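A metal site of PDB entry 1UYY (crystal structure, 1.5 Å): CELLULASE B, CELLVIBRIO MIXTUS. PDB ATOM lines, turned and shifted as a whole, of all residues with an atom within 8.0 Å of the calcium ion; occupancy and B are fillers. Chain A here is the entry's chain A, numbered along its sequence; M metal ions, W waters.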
ATOM      1  N   GLN A  14     -12.290  16.988  12.492  1.00  0.00           N
ATOM      2  CA  GLN A  14     -12.233  16.796  13.944  1.00  0.00           C
ATOM      3  C   GLN A  14     -11.313  15.648  14.302  1.00  0.00           C
ATOM      4  O   GLN A  14     -10.954  14.848  13.436  1.00  0.00           O
ATOM      5  CB  GLN A  14     -13.625  16.549  14.529  1.00  0.00           C
ATOM      6  CG  GLN A  14     -14.236  15.177  14.212  1.00  0.00           C
ATOM      7  CD  GLN A  14     -13.743  14.080  15.155  1.00  0.00           C
ATOM      8  OE1 GLN A  14     -13.731  14.256  16.350  1.00  0.00           O
ATOM      9  NE2 GLN A  14     -13.320  12.959  14.585  1.00  0.00           N
ATOM     10  N   SER A  15     -10.957  15.561  15.577  1.00  0.00           N
ATOM     11  CA  SER A  15     -10.233  14.411  16.117  1.00  0.00           C
ATOM     12  C   SER A  15     -10.750  14.031  17.500  1.00  0.00           C
ATOM     13  O   SER A  15     -10.808  14.861  18.391  1.00  0.00           O
ATOM     14  CB  SER A  15      -8.730  14.687  16.175  1.00  0.00           C
ATOM     15  OG  SER A  15      -8.026  13.509  16.577  1.00  0.00           O
ATOM     16  N   GLY A  16     -11.124  12.762  17.654  1.00  0.00           N
ATOM     17  CA  GLY A  16     -11.402  12.171  18.954  1.00  0.00           C
ATOM     18  C   GLY A  16     -12.799  12.286  19.533  1.00  0.00           C
ATOM     19  O   GLY A  16     -13.038  11.761  20.627  1.00  0.00           O
ATOM     20  N   THR A  17     -13.722  12.947  18.848  1.00  0.00           N
ATOM     21  CA  THR A  17     -15.040  13.258  19.415  1.00  0.00           C
ATOM     22  C   THR A  17     -16.142  12.561  18.661  1.00  0.00           C
ATOM     23  O   THR A  17     -15.904  11.936  17.630  1.00  0.00           O
ATOM     24  CB  THR A  17     -15.312  14.790  19.426  1.00  0.00           C
ATOM     25  OG1 THR A  17     -15.567  15.280  18.099  1.00  0.00           O
ATOM     26  CG2 THR A  17     -14.096  15.558  19.929  1.00  0.00           C
ATOM     27  N   GLN A  18     -17.371  12.709  19.164  1.00  0.00           N
ATOM     28  CA  GLN A  18     -18.547  12.261  18.451  1.00  0.00           C
ATOM     29  C   GLN A  18     -19.745  13.130  18.797  1.00  0.00           C
ATOM     30  O   GLN A  18     -19.862  13.656  19.897  1.00  0.00           O
ATOM     31  CB  GLN A  18     -18.860  10.798  18.758  1.00  0.00           C
ATOM     32  CG  GLN A  18     -19.519  10.567  20.093  1.00  0.00           C
ATOM     33  CD  GLN A  18     -19.966   9.134  20.326  1.00  0.00           C
ATOM     34  OE1 GLN A  18     -21.019   8.713  19.851  1.00  0.00           O
ATOM     35  NE2 GLN A  18     -19.162   8.375  21.068  1.00  0.00           N
ATOM     36  N   GLY A  32     -19.597  15.596  21.945  1.00  0.00           N
ATOM     37  CA  GLY A  32     -19.292  14.916  23.189  1.00  0.00           C
ATOM     38  C   GLY A  32     -18.053  14.055  23.082  1.00  0.00           C
ATOM     39  O   GLY A  32     -17.349  14.036  22.059  1.00  0.00           O
ATOM     40  N   TYR A  33     -17.777  13.328  24.165  1.00  0.00           N
ATOM     41  CA  TYR A  33     -16.596  12.479  24.288  1.00  0.00           C
ATOM     42  C   TYR A  33     -15.306  13.227  23.972  1.00  0.00           C
ATOM     43  O   TYR A  33     -14.475  12.803  23.162  1.00  0.00           O
ATOM     44  CB  TYR A  33     -16.773  11.192  23.477  1.00  0.00           C
ATOM     45  CG  TYR A  33     -17.968  10.425  23.977  1.00  0.00           C
ATOM     46  CD1 TYR A  33     -19.232  10.644  23.450  1.00  0.00           C
ATOM     47  CD2 TYR A  33     -17.847   9.555  25.049  1.00  0.00           C
ATOM     48  CE1 TYR A  33     -20.342   9.974  23.933  1.00  0.00           C
ATOM     49  CE2 TYR A  33     -18.959   8.877  25.552  1.00  0.00           C
ATOM     50  CZ  TYR A  33     -20.199   9.104  24.978  1.00  0.00           C
ATOM     51  OH  TYR A  33     -21.317   8.456  25.454  1.00  0.00           O
ATOM     52  N   ILE A  34     -15.173  14.373  24.638  1.00  0.00           N
ATOM     53  CA  ILE A  34     -14.032  15.274  24.502  1.00  0.00           C
ATOM     54  C   ILE A  34     -12.986  14.951  25.575  1.00  0.00           C
ATOM     55  O   ILE A  34     -13.307  14.814  26.757  1.00  0.00           O
ATOM     56  CB  ILE A  34     -14.503  16.753  24.594  1.00  0.00           C
ATOM     57  CG1 ILE A  34     -15.614  17.026  23.563  1.00  0.00           C
ATOM     58  CG2 ILE A  34     -13.306  17.696  24.407  1.00  0.00           C
ATOM     59  CD1 ILE A  34     -16.128  18.469  23.550  1.00  0.00           C
ATOM     60  N   ASP A  35     -11.741  14.814  25.131  1.00  0.00           N
ATOM     61  CA  ASP A  35     -10.609  14.470  25.996  1.00  0.00           C
ATOM     62  C   ASP A  35      -9.389  15.289  25.586  1.00  0.00           C
ATOM     63  O   ASP A  35      -9.340  15.828  24.485  1.00  0.00           O
ATOM     64  CB  ASP A  35     -10.246  12.990  25.860  1.00  0.00           C
ATOM     65  CG  ASP A  35     -11.422  12.074  26.050  1.00  0.00           C
ATOM     66  OD1 ASP A  35     -11.603  11.560  27.176  1.00  0.00           O
ATOM     67  OD2 ASP A  35     -12.211  11.821  25.122  1.00  0.00           O
ATOM     68  N   ALA A  36      -8.372  15.311  26.437  1.00  0.00           N
ATOM     69  CA  ALA A  36      -7.107  15.960  26.129  1.00  0.00           C
ATOM     70  C   ALA A  36      -6.537  15.493  24.792  1.00  0.00           C
ATOM     71  O   ALA A  36      -6.376  14.287  24.573  1.00  0.00           O
ATOM     72  CB  ALA A  36      -6.112  15.702  27.236  1.00  0.00           C
ATOM     73  N   GLY A  37      -6.218  16.444  23.923  1.00  0.00           N
ATOM     74  CA  GLY A  37      -5.691  16.184  22.598  1.00  0.00           C
ATOM     75  C   GLY A  37      -6.722  16.288  21.481  1.00  0.00           C
ATOM     76  O   GLY A  37      -6.369  16.522  20.320  1.00  0.00           O
ATOM     77  N   ASP A  38      -7.992  16.105  21.824  1.00  0.00           N
ATOM     78  CA  ASP A  38      -9.065  16.170  20.837  1.00  0.00           C
ATOM     79  C   ASP A  38      -9.205  17.589  20.292  1.00  0.00           C
ATOM     80  O   ASP A  38      -8.808  18.549  20.950  1.00  0.00           O
ATOM     81  CB  ASP A  38     -10.395  15.749  21.448  1.00  0.00           C
ATOM     82  CG  ASP A  38     -10.452  14.275  21.803  1.00  0.00           C
ATOM     83  OD1 ASP A  38      -9.521  13.494  21.447  1.00  0.00           O
ATOM     84  OD2 ASP A  38     -11.415  13.812  22.442  1.00  0.00           O
ATOM     85  N   TRP A  39      -9.746  17.730  19.083  1.00  0.00           N
ATOM     86  CA  TRP A  39      -9.906  19.047  18.482  1.00  0.00           C
ATOM     87  C   TRP A  39     -11.027  19.093  17.455  1.00  0.00           C
ATOM     88  O   TRP A  39     -11.502  18.070  16.987  1.00  0.00           O
ATOM     89  CB  TRP A  39      -8.582  19.545  17.867  1.00  0.00           C
ATOM     90  CG  TRP A  39      -7.926  18.627  16.864  1.00  0.00           C
ATOM     91  CD1 TRP A  39      -6.884  17.778  17.103  1.00  0.00           C
ATOM     92  CD2 TRP A  39      -8.220  18.520  15.472  1.00  0.00           C
ATOM     93  NE1 TRP A  39      -6.525  17.141  15.939  1.00  0.00           N
ATOM     94  CE2 TRP A  39      -7.331  17.572  14.927  1.00  0.00           C
ATOM     95  CE3 TRP A  39      -9.152  19.119  14.613  1.00  0.00           C
ATOM     96  CZ2 TRP A  39      -7.347  17.212  13.574  1.00  0.00           C
ATOM     97  CZ3 TRP A  39      -9.169  18.758  13.274  1.00  0.00           C
ATOM     98  CH2 TRP A  39      -8.273  17.815  12.766  1.00  0.00           C
ATOM     99  N   ALA A 115      -8.947  20.776  22.785  1.00  0.00           N
ATOM    100  CA  ALA A 115      -9.214  20.421  24.182  1.00  0.00           C
ATOM    101  C   ALA A 115      -7.919  20.113  24.914  1.00  0.00           C
ATOM    102  O   ALA A 115      -7.193  19.198  24.549  1.00  0.00           O
ATOM    103  CB  ALA A 115     -10.150  19.233  24.251  1.00  0.00           C
ATOM    104  N   GLY A 118     -10.391  17.134  29.102  1.00  0.00           N
ATOM    105  CA  GLY A 118     -11.765  16.773  28.788  1.00  0.00           C
ATOM    106  C   GLY A 118     -12.742  16.980  29.925  1.00  0.00           C
ATOM    107  O   GLY A 118     -12.485  17.748  30.861  1.00  0.00           O
HETATM  108 CA    CA M   1     -12.454  11.733  22.846  1.00  0.00          CA
HETATM  109  O   HOH W   1     -13.079   9.575  23.558  1.00  0.00           O
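N of Gly 16 is in hydrogen-bond range of OE1 of Gln 14, 3.3 Å away. The backbone carbonyl oxygen (O) of Asp 38 lies within hydrogen-bond range of the backbone NH (N) of Ala 115, at 2.9 Å.
Within 4 Å of the calcium ion: Gly 16, Tyr 33, Asp 35 and Asp 38. The nearest printed residue that does not touch the calcium ion is Ile 34 (4.2 Å).
The calcium ion is bound by OD2 of Asp 35 (2.3 Å), O of Gly 16 (2.3 Å), O of Tyr 33 (2.3 Å), water W1 (2.4 Å) and OD2 of Asp 38 (2.4 Å).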
